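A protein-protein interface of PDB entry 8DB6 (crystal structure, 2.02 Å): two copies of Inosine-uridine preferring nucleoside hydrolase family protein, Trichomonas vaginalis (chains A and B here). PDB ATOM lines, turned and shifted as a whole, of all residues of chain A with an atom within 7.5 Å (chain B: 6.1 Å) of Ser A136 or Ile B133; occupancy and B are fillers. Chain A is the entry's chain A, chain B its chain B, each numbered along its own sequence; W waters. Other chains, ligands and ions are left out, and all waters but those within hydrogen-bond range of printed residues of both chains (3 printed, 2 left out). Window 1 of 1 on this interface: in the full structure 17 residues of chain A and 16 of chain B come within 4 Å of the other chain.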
ATOM      1  N   CYS A  65      19.280   0.995  29.973  1.00  0.00           N
ATOM      2  CA  CYS A  65      18.383   1.501  30.997  1.00  0.00           C
ATOM      3  C   CYS A  65      18.343   0.537  32.189  1.00  0.00           C
ATOM      4  O   CYS A  65      18.522  -0.678  32.040  1.00  0.00           O
ATOM      5  CB  CYS A  65      16.983   1.694  30.395  1.00  0.00           C
ATOM      6  SG  CYS A  65      16.948   2.780  28.895  1.00  0.00           S
ATOM      7  N   LEU A  69      10.219   0.848  30.958  1.00  0.00           N
ATOM      8  CA  LEU A  69       9.753   2.210  30.692  1.00  0.00           C
ATOM      9  C   LEU A  69       8.852   2.719  31.808  1.00  0.00           C
ATOM     10  O   LEU A  69       9.123   3.769  32.394  1.00  0.00           O
ATOM     11  CB  LEU A  69       9.019   2.280  29.360  1.00  0.00           C
ATOM     12  CG  LEU A  69       9.907   2.116  28.128  1.00  0.00           C
ATOM     13  CD1 LEU A  69       9.059   2.209  26.864  1.00  0.00           C
ATOM     14  CD2 LEU A  69      11.024   3.164  28.136  1.00  0.00           C
ATOM     15  N   HIS A 105      26.121   5.266  26.383  1.00  0.00           N
ATOM     16  CA  HIS A 105      24.878   4.570  26.686  1.00  0.00           C
ATOM     17  C   HIS A 105      24.500   3.667  25.519  1.00  0.00           C
ATOM     18  O   HIS A 105      24.675   4.029  24.352  1.00  0.00           O
ATOM     19  CB  HIS A 105      23.761   5.584  26.966  1.00  0.00           C
ATOM     20  CG  HIS A 105      22.525   4.989  27.565  1.00  0.00           C
ATOM     21  ND1 HIS A 105      21.575   4.332  26.814  1.00  0.00           N
ATOM     22  CD2 HIS A 105      22.068   4.978  28.841  1.00  0.00           C
ATOM     23  CE1 HIS A 105      20.595   3.925  27.605  1.00  0.00           C
ATOM     24  NE2 HIS A 105      20.865   4.315  28.836  1.00  0.00           N
ATOM     25  N   VAL A 107      21.762   3.074  24.159  1.00  0.00           N
ATOM     26  CA  VAL A 107      20.824   3.660  23.195  1.00  0.00           C
ATOM     27  C   VAL A 107      21.578   4.437  22.120  1.00  0.00           C
ATOM     28  O   VAL A 107      21.345   4.258  20.919  1.00  0.00           O
ATOM     29  CB  VAL A 107      19.784   4.544  23.913  1.00  0.00           C
ATOM     30  CG1 VAL A 107      19.006   5.387  22.902  1.00  0.00           C
ATOM     31  CG2 VAL A 107      18.807   3.673  24.736  1.00  0.00           C
ATOM     32  N   ILE A 111      22.129   3.532  18.129  1.00  0.00           N
ATOM     33  CA  ILE A 111      21.811   4.477  17.058  1.00  0.00           C
ATOM     34  C   ILE A 111      23.017   4.675  16.148  1.00  0.00           C
ATOM     35  O   ILE A 111      22.893   4.680  14.916  1.00  0.00           O
ATOM     36  CB  ILE A 111      21.303   5.804  17.649  1.00  0.00           C
ATOM     37  CG1 ILE A 111      19.896   5.592  18.243  1.00  0.00           C
ATOM     38  CG2 ILE A 111      21.250   6.888  16.587  1.00  0.00           C
ATOM     39  CD1 ILE A 111      19.502   6.628  19.286  1.00  0.00           C
ATOM     40  N   THR A 129      13.189  -2.456  26.290  1.00  0.00           N
ATOM     41  CA  THR A 129      13.361  -1.085  26.785  1.00  0.00           C
ATOM     42  C   THR A 129      14.375  -0.272  25.988  1.00  0.00           C
ATOM     43  O   THR A 129      14.068   0.838  25.530  1.00  0.00           O
ATOM     44  CB  THR A 129      13.779  -1.127  28.253  1.00  0.00           C
ATOM     45  OG1 THR A 129      12.987  -2.099  28.939  1.00  0.00           O
ATOM     46  CG2 THR A 129      13.599   0.261  28.919  1.00  0.00           C
ATOM     47  N   ASN A 130      15.604  -0.792  25.852  1.00  0.00           N
ATOM     48  CA  ASN A 130      16.653  -0.090  25.108  1.00  0.00           C
ATOM     49  C   ASN A 130      16.257   0.138  23.663  1.00  0.00           C
ATOM     50  O   ASN A 130      16.538   1.197  23.093  1.00  0.00           O
ATOM     51  CB  ASN A 130      17.963  -0.886  25.120  1.00  0.00           C
ATOM     52  CG  ASN A 130      18.619  -0.926  26.456  1.00  0.00           C
ATOM     53  OD1 ASN A 130      18.431  -0.039  27.288  1.00  0.00           O
ATOM     54  ND2 ASN A 130      19.444  -1.955  26.671  1.00  0.00           N
ATOM     55  N   ILE A 131      15.652  -0.864  23.030  1.00  0.00           N
ATOM     56  CA  ILE A 131      15.302  -0.730  21.623  1.00  0.00           C
ATOM     57  C   ILE A 131      14.191   0.287  21.452  1.00  0.00           C
ATOM     58  O   ILE A 131      14.189   1.074  20.493  1.00  0.00           O
ATOM     59  CB  ILE A 131      14.882  -2.088  21.037  1.00  0.00           C
ATOM     60  CG1 ILE A 131      15.868  -3.181  21.473  1.00  0.00           C
ATOM     61  CG2 ILE A 131      14.727  -1.954  19.510  1.00  0.00           C
ATOM     62  CD1 ILE A 131      17.308  -2.837  21.167  1.00  0.00           C
ATOM     63  N   ALA A 132      13.213   0.248  22.364  1.00  0.00           N
ATOM     64  CA  ALA A 132      12.094   1.172  22.322  1.00  0.00           C
ATOM     65  C   ALA A 132      12.559   2.608  22.511  1.00  0.00           C
ATOM     66  O   ALA A 132      12.007   3.509  21.887  1.00  0.00           O
ATOM     67  CB  ALA A 132      11.058   0.813  23.391  1.00  0.00           C
ATOM     68  N   ILE A 133      13.554   2.849  23.377  1.00  0.00           N
ATOM     69  CA  ILE A 133      14.079   4.208  23.551  1.00  0.00           C
ATOM     70  C   ILE A 133      14.838   4.655  22.304  1.00  0.00           C
ATOM     71  O   ILE A 133      14.665   5.789  21.835  1.00  0.00           O
ATOM     72  CB  ILE A 133      14.941   4.296  24.827  1.00  0.00           C
ATOM     73  CG1 ILE A 133      14.073   4.075  26.078  1.00  0.00           C
ATOM     74  CG2 ILE A 133      15.665   5.650  24.914  1.00  0.00           C
ATOM     75  CD1 ILE A 133      13.223   5.228  26.417  1.00  0.00           C
ATOM     76  N   ALA A 134      15.607   3.745  21.687  1.00  0.00           N
ATOM     77  CA  ALA A 134      16.318   4.085  20.460  1.00  0.00           C
ATOM     78  C   ALA A 134      15.353   4.431  19.323  1.00  0.00           C
ATOM     79  O   ALA A 134      15.628   5.336  18.523  1.00  0.00           O
ATOM     80  CB  ALA A 134      17.261   2.940  20.048  1.00  0.00           C
ATOM     81  N   LEU A 135      14.214   3.740  19.232  1.00  0.00           N
ATOM     82  CA  LEU A 135      13.293   4.006  18.125  1.00  0.00           C
ATOM     83  C   LEU A 135      12.569   5.357  18.287  1.00  0.00           C
ATOM     84  O   LEU A 135      12.205   5.997  17.300  1.00  0.00           O
ATOM     85  CB  LEU A 135      12.276   2.863  18.024  1.00  0.00           C
ATOM     86  CG  LEU A 135      12.694   1.563  17.314  1.00  0.00           C
ATOM     87  CD1 LEU A 135      11.871   0.393  17.832  1.00  0.00           C
ATOM     88  CD2 LEU A 135      12.502   1.691  15.811  1.00  0.00           C
ATOM     89  N   SER A 136      12.331   5.780  19.523  1.00  0.00           N
ATOM     90  CA  SER A 136      11.710   7.069  19.832  1.00  0.00           C
ATOM     91  C   SER A 136      12.665   8.227  19.579  1.00  0.00           C
ATOM     92  O   SER A 136      12.238   9.292  19.116  1.00  0.00           O
ATOM     93  CB  SER A 136      11.263   7.090  21.301  1.00  0.00           C
ATOM     94  OG  SER A 136      10.674   5.852  21.690  1.00  0.00           O
ATOM     95  N   MET A 137      13.947   8.033  19.891  1.00  0.00           N
ATOM     96  CA  MET A 137      14.951   9.074  19.728  1.00  0.00           C
ATOM     97  C   MET A 137      15.383   9.235  18.279  1.00  0.00           C
ATOM     98  O   MET A 137      15.624  10.356  17.818  1.00  0.00           O
ATOM     99  CB  MET A 137      16.165   8.767  20.594  1.00  0.00           C
ATOM    100  CG  MET A 137      15.891   9.067  22.033  1.00  0.00           C
ATOM    101  SD  MET A 137      17.355   9.104  23.043  1.00  0.00           S
ATOM    102  CE  MET A 137      18.313  10.442  22.278  1.00  0.00           C
ATOM    103  N   ALA A 138      15.506   8.148  17.533  1.00  0.00           N
ATOM    104  CA  ALA A 138      16.034   8.224  16.174  1.00  0.00           C
ATOM    105  C   ALA A 138      15.436   7.107  15.330  1.00  0.00           C
ATOM    106  O   ALA A 138      16.149   6.219  14.843  1.00  0.00           O
ATOM    107  CB  ALA A 138      17.562   8.166  16.192  1.00  0.00           C
ATOM    108  N   PRO A 139      14.118   7.137  15.114  1.00  0.00           N
ATOM    109  CA  PRO A 139      13.510   6.119  14.245  1.00  0.00           C
ATOM    110  C   PRO A 139      14.222   5.988  12.907  1.00  0.00           C
ATOM    111  O   PRO A 139      14.388   4.872  12.393  1.00  0.00           O
ATOM    112  CB  PRO A 139      12.066   6.616  14.074  1.00  0.00           C
ATOM    113  CG  PRO A 139      12.123   8.106  14.381  1.00  0.00           C
ATOM    114  CD  PRO A 139      13.188   8.243  15.425  1.00  0.00           C
ATOM    115  N   GLU A 140      14.690   7.104  12.343  1.00  0.00           N
ATOM    116  CA  GLU A 140      15.323   7.047  11.034  1.00  0.00           C
ATOM    117  C   GLU A 140      16.598   6.206  11.080  1.00  0.00           C
ATOM    118  O   GLU A 140      16.918   5.505  10.116  1.00  0.00           O
ATOM    119  CB  GLU A 140      15.607   8.462  10.517  1.00  0.00           C
ATOM    120  CG  GLU A 140      16.735   9.187  11.240  1.00  0.00           C
ATOM    121  CD  GLU A 140      16.340   9.724  12.615  1.00  0.00           C
ATOM    122  OE1 GLU A 140      17.265  10.181  13.325  1.00  0.00           O
ATOM    123  OE2 GLU A 140      15.127   9.710  12.972  1.00  0.00           O
ATOM    124  N   ILE A 142      17.274   3.625  13.458  1.00  0.00           N
ATOM    125  CA  ILE A 142      16.960   2.226  13.747  1.00  0.00           C
ATOM    126  C   ILE A 142      16.301   1.548  12.555  1.00  0.00           C
ATOM    127  O   ILE A 142      16.473   0.341  12.350  1.00  0.00           O
ATOM    128  CB  ILE A 142      16.089   2.104  15.009  1.00  0.00           C
ATOM    129  CG1 ILE A 142      16.792   2.771  16.175  1.00  0.00           C
ATOM    130  CG2 ILE A 142      15.823   0.647  15.344  1.00  0.00           C
ATOM    131  CD1 ILE A 142      18.234   2.339  16.331  1.00  0.00           C
ATOM    132  N   ILE A 178       6.001  -0.189  21.278  1.00  0.00           N
ATOM    133  CA  ILE A 178       6.781   0.788  20.516  1.00  0.00           C
ATOM    134  C   ILE A 178       7.554   0.101  19.395  1.00  0.00           C
ATOM    135  O   ILE A 178       7.618   0.596  18.263  1.00  0.00           O
ATOM    136  CB  ILE A 178       7.730   1.558  21.459  1.00  0.00           C
ATOM    137  CG1 ILE A 178       6.947   2.589  22.274  1.00  0.00           C
ATOM    138  CG2 ILE A 178       8.865   2.228  20.679  1.00  0.00           C
ATOM    139  CD1 ILE A 178       7.729   3.069  23.517  1.00  0.00           C
ATOM    140  N   THR A 182       6.640   0.675  15.431  1.00  0.00           N
ATOM    141  CA  THR A 182       7.609   1.546  14.772  1.00  0.00           C
ATOM    142  C   THR A 182       8.542   0.792  13.826  1.00  0.00           C
ATOM    143  O   THR A 182       8.773   1.238  12.701  1.00  0.00           O
ATOM    144  CB  THR A 182       8.427   2.286  15.839  1.00  0.00           C
ATOM    145  OG1 THR A 182       7.537   2.777  16.860  1.00  0.00           O
ATOM    146  CG2 THR A 182       9.196   3.432  15.239  1.00  0.00           C
ATOM    147  N   GLY B  64      13.242  17.460  19.777  1.00  0.00           N
ATOM    148  CA  GLY B  64      13.084  16.250  20.570  1.00  0.00           C
ATOM    149  C   GLY B  64      12.337  15.164  19.831  1.00  0.00           C
ATOM    150  O   GLY B  64      12.526  14.961  18.621  1.00  0.00           O
ATOM    151  N   CYS B  65      11.452  14.469  20.552  1.00  0.00           N
ATOM    152  CA  CYS B  65      10.839  13.309  19.921  1.00  0.00           C
ATOM    153  C   CYS B  65       9.753  13.717  18.917  1.00  0.00           C
ATOM    154  O   CYS B  65       9.292  14.867  18.879  1.00  0.00           O
ATOM    155  CB  CYS B  65      10.298  12.358  20.982  1.00  0.00           C
ATOM    156  SG  CYS B  65      11.679  11.662  21.956  1.00  0.00           S
ATOM    157  N   GLN B  66       9.384  12.752  18.063  1.00  0.00           N
ATOM    158  CA  GLN B  66       8.424  12.944  16.983  1.00  0.00           C
ATOM    159  C   GLN B  66       7.029  12.446  17.326  1.00  0.00           C
ATOM    160  O   GLN B  66       6.103  12.645  16.535  1.00  0.00           O
ATOM    161  CB  GLN B  66       8.902  12.240  15.709  1.00  0.00           C
ATOM    162  CG  GLN B  66      10.349  12.502  15.383  1.00  0.00           C
ATOM    163  CD  GLN B  66      10.664  12.290  13.910  1.00  0.00           C
ATOM    164  OE1 GLN B  66       9.839  12.582  13.039  1.00  0.00           O
ATOM    165  NE2 GLN B  66      11.852  11.747  13.627  1.00  0.00           N
ATOM    166  N   ALA B  67       6.846  11.835  18.485  1.00  0.00           N
ATOM    167  CA  ALA B  67       5.567  11.245  18.835  1.00  0.00           C
ATOM    168  C   ALA B  67       5.572  11.000  20.331  1.00  0.00           C
ATOM    169  O   ALA B  67       6.641  11.010  20.958  1.00  0.00           O
ATOM    170  CB  ALA B  67       5.335   9.933  18.057  1.00  0.00           C
ATOM    171  N   PRO B  68       4.402  10.774  20.934  1.00  0.00           N
ATOM    172  CA  PRO B  68       4.362  10.377  22.339  1.00  0.00           C
ATOM    173  C   PRO B  68       5.081   9.055  22.506  1.00  0.00           C
ATOM    174  O   PRO B  68       5.306   8.323  21.541  1.00  0.00           O
ATOM    175  CB  PRO B  68       2.860  10.240  22.641  1.00  0.00           C
ATOM    176  CG  PRO B  68       2.172  10.971  21.525  1.00  0.00           C
ATOM    177  CD  PRO B  68       3.053  10.787  20.336  1.00  0.00           C
ATOM    178  N   LEU B  69       5.452   8.764  23.750  1.00  0.00           N
ATOM    179  CA  LEU B  69       6.210   7.553  24.038  1.00  0.00           C
ATOM    180  C   LEU B  69       5.546   6.330  23.414  1.00  0.00           C
ATOM    181  O   LEU B  69       6.170   5.608  22.632  1.00  0.00           O
ATOM    182  CB  LEU B  69       6.370   7.389  25.545  1.00  0.00           C
ATOM    183  CG  LEU B  69       7.398   6.356  25.977  1.00  0.00           C
ATOM    184  CD1 LEU B  69       8.772   6.711  25.427  1.00  0.00           C
ATOM    185  CD2 LEU B  69       7.414   6.237  27.500  1.00  0.00           C
ATOM    186  N   HIS B 105      20.004  15.854  19.483  1.00  0.00           N
ATOM    187  CA  HIS B 105      18.642  15.563  19.931  1.00  0.00           C
ATOM    188  C   HIS B 105      18.406  16.180  21.301  1.00  0.00           C
ATOM    189  O   HIS B 105      19.313  16.226  22.136  1.00  0.00           O
ATOM    190  CB  HIS B 105      18.439  14.042  20.002  1.00  0.00           C
ATOM    191  CG  HIS B 105      17.011  13.612  20.158  1.00  0.00           C
ATOM    192  ND1 HIS B 105      16.336  13.686  21.356  1.00  0.00           N
ATOM    193  CD2 HIS B 105      16.140  13.076  19.268  1.00  0.00           C
ATOM    194  CE1 HIS B 105      15.105  13.224  21.197  1.00  0.00           C
ATOM    195  NE2 HIS B 105      14.961  12.845  19.939  1.00  0.00           N
ATOM    196  N   VAL B 107      16.864  15.155  23.929  1.00  0.00           N
ATOM    197  CA  VAL B 107      17.095  14.280  25.078  1.00  0.00           C
ATOM    198  C   VAL B 107      18.562  14.315  25.483  1.00  0.00           C
ATOM    199  O   VAL B 107      18.896  14.533  26.656  1.00  0.00           O
ATOM    200  CB  VAL B 107      16.624  12.847  24.765  1.00  0.00           C
ATOM    201  CG1 VAL B 107      17.048  11.909  25.865  1.00  0.00           C
ATOM    202  CG2 VAL B 107      15.100  12.808  24.618  1.00  0.00           C
ATOM    203  N   ILE B 111      20.231  15.888  28.995  1.00  0.00           N
ATOM    204  CA  ILE B 111      21.146  15.122  29.838  1.00  0.00           C
ATOM    205  C   ILE B 111      22.466  15.864  30.001  1.00  0.00           C
ATOM    206  O   ILE B 111      22.974  16.024  31.118  1.00  0.00           O
ATOM    207  CB  ILE B 111      21.359  13.721  29.245  1.00  0.00           C
ATOM    208  CG1 ILE B 111      20.069  12.907  29.384  1.00  0.00           C
ATOM    209  CG2 ILE B 111      22.543  13.037  29.913  1.00  0.00           C
ATOM    210  CD1 ILE B 111      20.011  11.666  28.499  1.00  0.00           C
ATOM    211  N   LEU B 128       5.304  15.240  28.354  1.00  0.00           N
ATOM    212  CA  LEU B 128       6.596  15.118  28.995  1.00  0.00           C
ATOM    213  C   LEU B 128       7.509  14.096  28.297  1.00  0.00           C
ATOM    214  O   LEU B 128       8.481  13.635  28.899  1.00  0.00           O
ATOM    215  CB  LEU B 128       6.392  14.772  30.471  1.00  0.00           C
ATOM    216  CG  LEU B 128       5.705  15.882  31.270  1.00  0.00           C
ATOM    217  CD1 LEU B 128       5.134  15.357  32.565  1.00  0.00           C
ATOM    218  CD2 LEU B 128       6.724  16.981  31.551  1.00  0.00           C
ATOM    219  N   THR B 129       7.221  13.776  27.037  1.00  0.00           N
ATOM    220  CA  THR B 129       7.949  12.742  26.291  1.00  0.00           C
ATOM    221  C   THR B 129       9.471  12.913  26.351  1.00  0.00           C
ATOM    222  O   THR B 129      10.192  11.971  26.690  1.00  0.00           O
ATOM    223  CB  THR B 129       7.476  12.757  24.837  1.00  0.00           C
ATOM    224  OG1 THR B 129       6.046  12.887  24.792  1.00  0.00           O
ATOM    225  CG2 THR B 129       7.914  11.512  24.102  1.00  0.00           C
ATOM    226  N   ASN B 130       9.985  14.100  25.989  1.00  0.00           N
ATOM    227  CA  ASN B 130      11.432  14.307  26.034  1.00  0.00           C
ATOM    228  C   ASN B 130      11.985  14.066  27.433  1.00  0.00           C
ATOM    229  O   ASN B 130      13.054  13.463  27.591  1.00  0.00           O
ATOM    230  CB  ASN B 130      11.805  15.720  25.586  1.00  0.00           C
ATOM    231  CG  ASN B 130      11.545  15.963  24.118  1.00  0.00           C
ATOM    232  OD1 ASN B 130      11.555  15.042  23.310  1.00  0.00           O
ATOM    233  ND2 ASN B 130      11.307  17.223  23.763  1.00  0.00           N
ATOM    234  N   ILE B 131      11.273  14.532  28.460  1.00  0.00           N
ATOM    235  CA  ILE B 131      11.796  14.447  29.824  1.00  0.00           C
ATOM    236  C   ILE B 131      11.799  12.998  30.313  1.00  0.00           C
ATOM    237  O   ILE B 131      12.739  12.559  30.985  1.00  0.00           O
ATOM    238  CB  ILE B 131      10.985  15.352  30.775  1.00  0.00           C
ATOM    239  CG1 ILE B 131      10.724  16.745  30.158  1.00  0.00           C
ATOM    240  CG2 ILE B 131      11.642  15.417  32.133  1.00  0.00           C
ATOM    241  CD1 ILE B 131      11.965  17.473  29.678  1.00  0.00           C
ATOM    242  N   ALA B 132      10.748  12.237  29.983  1.00  0.00           N
ATOM    243  CA  ALA B 132      10.635  10.865  30.451  1.00  0.00           C
ATOM    244  C   ALA B 132      11.688   9.969  29.809  1.00  0.00           C
ATOM    245  O   ALA B 132      12.173   9.025  30.439  1.00  0.00           O
ATOM    246  CB  ALA B 132       9.246  10.318  30.144  1.00  0.00           C
ATOM    247  N   ILE B 133      11.993  10.211  28.536  1.00  0.00           N
ATOM    248  CA  ILE B 133      13.056   9.469  27.866  1.00  0.00           C
ATOM    249  C   ILE B 133      14.402   9.799  28.490  1.00  0.00           C
ATOM    250  O   ILE B 133      15.194   8.897  28.786  1.00  0.00           O
ATOM    251  CB  ILE B 133      13.020   9.754  26.357  1.00  0.00           C
ATOM    252  CG1 ILE B 133      11.764   9.083  25.774  1.00  0.00           C
ATOM    253  CG2 ILE B 133      14.306   9.288  25.681  1.00  0.00           C
ATOM    254  CD1 ILE B 133      11.642   9.192  24.331  1.00  0.00           C
ATOM    255  N   ALA B 134      14.651  11.085  28.775  1.00  0.00           N
ATOM    256  CA  ALA B 134      15.899  11.459  29.443  1.00  0.00           C
ATOM    257  C   ALA B 134      16.005  10.808  30.814  1.00  0.00           C
ATOM    258  O   ALA B 134      17.095  10.379  31.222  1.00  0.00           O
ATOM    259  CB  ALA B 134      16.012  12.982  29.569  1.00  0.00           C
ATOM    260  N   LEU B 135      14.886  10.713  31.541  1.00  0.00           N
ATOM    261  CA  LEU B 135      14.904  10.039  32.838  1.00  0.00           C
ATOM    262  C   LEU B 135      15.107   8.536  32.690  1.00  0.00           C
ATOM    263  O   LEU B 135      15.691   7.902  33.581  1.00  0.00           O
ATOM    264  CB  LEU B 135      13.609  10.296  33.605  1.00  0.00           C
ATOM    265  CG  LEU B 135      13.489  11.634  34.355  1.00  0.00           C
ATOM    266  CD1 LEU B 135      12.011  12.014  34.535  1.00  0.00           C
ATOM    267  CD2 LEU B 135      14.199  11.586  35.704  1.00  0.00           C
ATOM    268  N   SER B 136      14.612   7.951  31.596  1.00  0.00           N
ATOM    269  CA  SER B 136      14.801   6.525  31.389  1.00  0.00           C
ATOM    270  C   SER B 136      16.255   6.220  31.061  1.00  0.00           C
ATOM    271  O   SER B 136      16.824   5.260  31.580  1.00  0.00           O
ATOM    272  CB  SER B 136      13.855   6.051  30.290  1.00  0.00           C
ATOM    273  OG  SER B 136      12.524   6.250  30.733  1.00  0.00           O
ATOM    274  N   MET B 137      16.882   7.046  30.240  1.00  0.00           N
ATOM    275  CA  MET B 137      18.261   6.807  29.817  1.00  0.00           C
ATOM    276  C   MET B 137      19.283   7.114  30.900  1.00  0.00           C
ATOM    277  O   MET B 137      20.271   6.376  31.054  1.00  0.00           O
ATOM    278  CB  MET B 137      18.580   7.650  28.582  1.00  0.00           C
ATOM    279  CG  MET B 137      18.014   7.033  27.352  1.00  0.00           C
ATOM    280  SD  MET B 137      18.372   8.083  25.970  1.00  0.00           S
ATOM    281  CE  MET B 137      20.179   8.009  25.970  1.00  0.00           C
ATOM    282  N   ALA B 138      19.093   8.219  31.619  1.00  0.00           N
ATOM    283  CA  ALA B 138      20.113   8.744  32.518  1.00  0.00           C
ATOM    284  C   ALA B 138      19.437   9.389  33.716  1.00  0.00           C
ATOM    285  O   ALA B 138      19.524  10.606  33.919  1.00  0.00           O
ATOM    286  CB  ALA B 138      20.999   9.746  31.784  1.00  0.00           C
ATOM    287  N   ILE B 178       6.213   8.444  34.249  1.00  0.00           N
ATOM    288  CA  ILE B 178       7.653   8.283  34.386  1.00  0.00           C
ATOM    289  C   ILE B 178       8.254   9.432  35.182  1.00  0.00           C
ATOM    290  O   ILE B 178       9.051   9.219  36.109  1.00  0.00           O
ATOM    291  CB  ILE B 178       8.308   8.147  33.002  1.00  0.00           C
ATOM    292  CG1 ILE B 178       7.976   6.763  32.424  1.00  0.00           C
ATOM    293  CG2 ILE B 178       9.796   8.262  33.142  1.00  0.00           C
ATOM    294  CD1 ILE B 178       8.356   6.602  30.992  1.00  0.00           C
HETATM  295  O   HOH W   1       9.767   9.757  18.546  1.00  0.00           O
HETATM  296  O   HOH W   2      11.533   4.850  32.637  1.00  0.00           O
HETATM  297  O   HOH W   3       8.055   6.372  20.669  1.00  0.00           O
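SG of Cys B65 lies within hydrogen-bond range of O of Ser A136 (3.7 Å). The backbone carbonyl oxygen (O) of Met A137 sits close to a ring nitrogen (NE2) of His B105 (3.3 Å). O of Ser B136 lies within hydrogen-bond range of SG of Cys A65. O of Met B137 is in hydrogen-bond range of NE2 of His A105. SD of Met B137 sits close to SD of Met A137, 3.3 Å away.
The side-chain amide oxygen (OD1) of Asn B130 sits at hydrogen-bond distance from the backbone NH (N) of Cys B65 (2.8 Å). A ring nitrogen (ND1) of His B105 sits at hydrogen-bond distance from the backbone NH of Val B107, 3.0 Å away. The side-chain hydroxyl (OG) of Ser B136 is in hydrogen-bond range of the backbone carbonyl oxygen (O) of Ala B132 (2.8 Å). The backbone NH (N) of Cys A65 lies within hydrogen-bond range of the side-chain amide oxygen (OD1) of Asn A130, at 3.0 Å. A ring nitrogen (ND1) of His A105 sits at hydrogen-bond distance from the backbone NH (N) of Val A107 (2.9 Å). The side-chain hydroxyl (OG1) of Thr A182 is in hydrogen-bond range of the backbone carbonyl oxygen (O) of Ile A178, at 2.6 Å.
Leu A69 touches Ile B178. Ile B133 touches Ile A133. Met B137 touches Ile A133 (CG to CG2, 3.7 Å). Ile B133 touches Ser A136. Met A137 touches Val B107 (CE to CB, 3.8 Å). CG of Met A137 touches CG2 of Ile B133, at 3.98 Å. CG of Pro A139 touches NE2 of Gln B66 (3.7 Å). OE2 of Glu A140 touches NE2 of Gln B66, at 3.9 Å. CD1 of Ile A178 touches O of Leu B69, at 3.1 Å.
Printed residues of chain B within 4 Å of Ile A178: Leu B69 (3.1 Å). Of the printed residues of chain A, Ile B133 touches Ile A133, Ser A136 and Met A137. Of the printed residues of chain A, Ser B136 touches Cys A65 (3.7 Å).
Of the 21 printed residues of chain B, 9 touch a printed residue of chain A. Hydrophobic or aromatic side chains of chain B that line the printed part of chain A: His B105, Val B107, Ile B133, Met B137 and Ile B178. Along chain B the printed residues that touch a printed residue of chain A span positions 65 to 178. Of the 20 printed residues of chain A, 9 touch a printed residue of chain B. Hydrophobic or aromatic side chains of chain A within 4 Å of the printed part of chain B: His A105, Ile A133, Met A137, Pro A139 and Ile A178. Among the printed residues, 14 pairs touch across the chains. Among the printed residues, no Asp or Glu carboxylate lies within 4 Å of a Lys or Arg side-chain nitrogen of the other chain.
Leu A69 touches Ile B178, and with the chains exchanged Ile A178 touches Leu B69. His A105 touches Met B137, and with the chains exchanged Met A137 touches His B105. Ile A133 touches its own counterpart, Ile B133. Met A137 touches its own counterpart, Met B137. Positions printed for both chains: 65, 69, 105, 107, 111, 129, 130, 131, 132, 133, 134, 135, 136, 137, 138 and 178.
Water W2 bridges the side-chain hydroxyl of Ser B136 (2.6 Å) and the backbone carbonyl oxygen of Leu A69 (2.7 Å). Water W1 bridges the backbone carbonyl oxygen (O) of Ser A136 and the backbone NH (N) of Gln B66. Water W3 lies within hydrogen-bond range of O of Leu B69 (2.8 Å), OG of Ser A136 (2.9 Å) and O of Pro B68 (3.5 Å).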
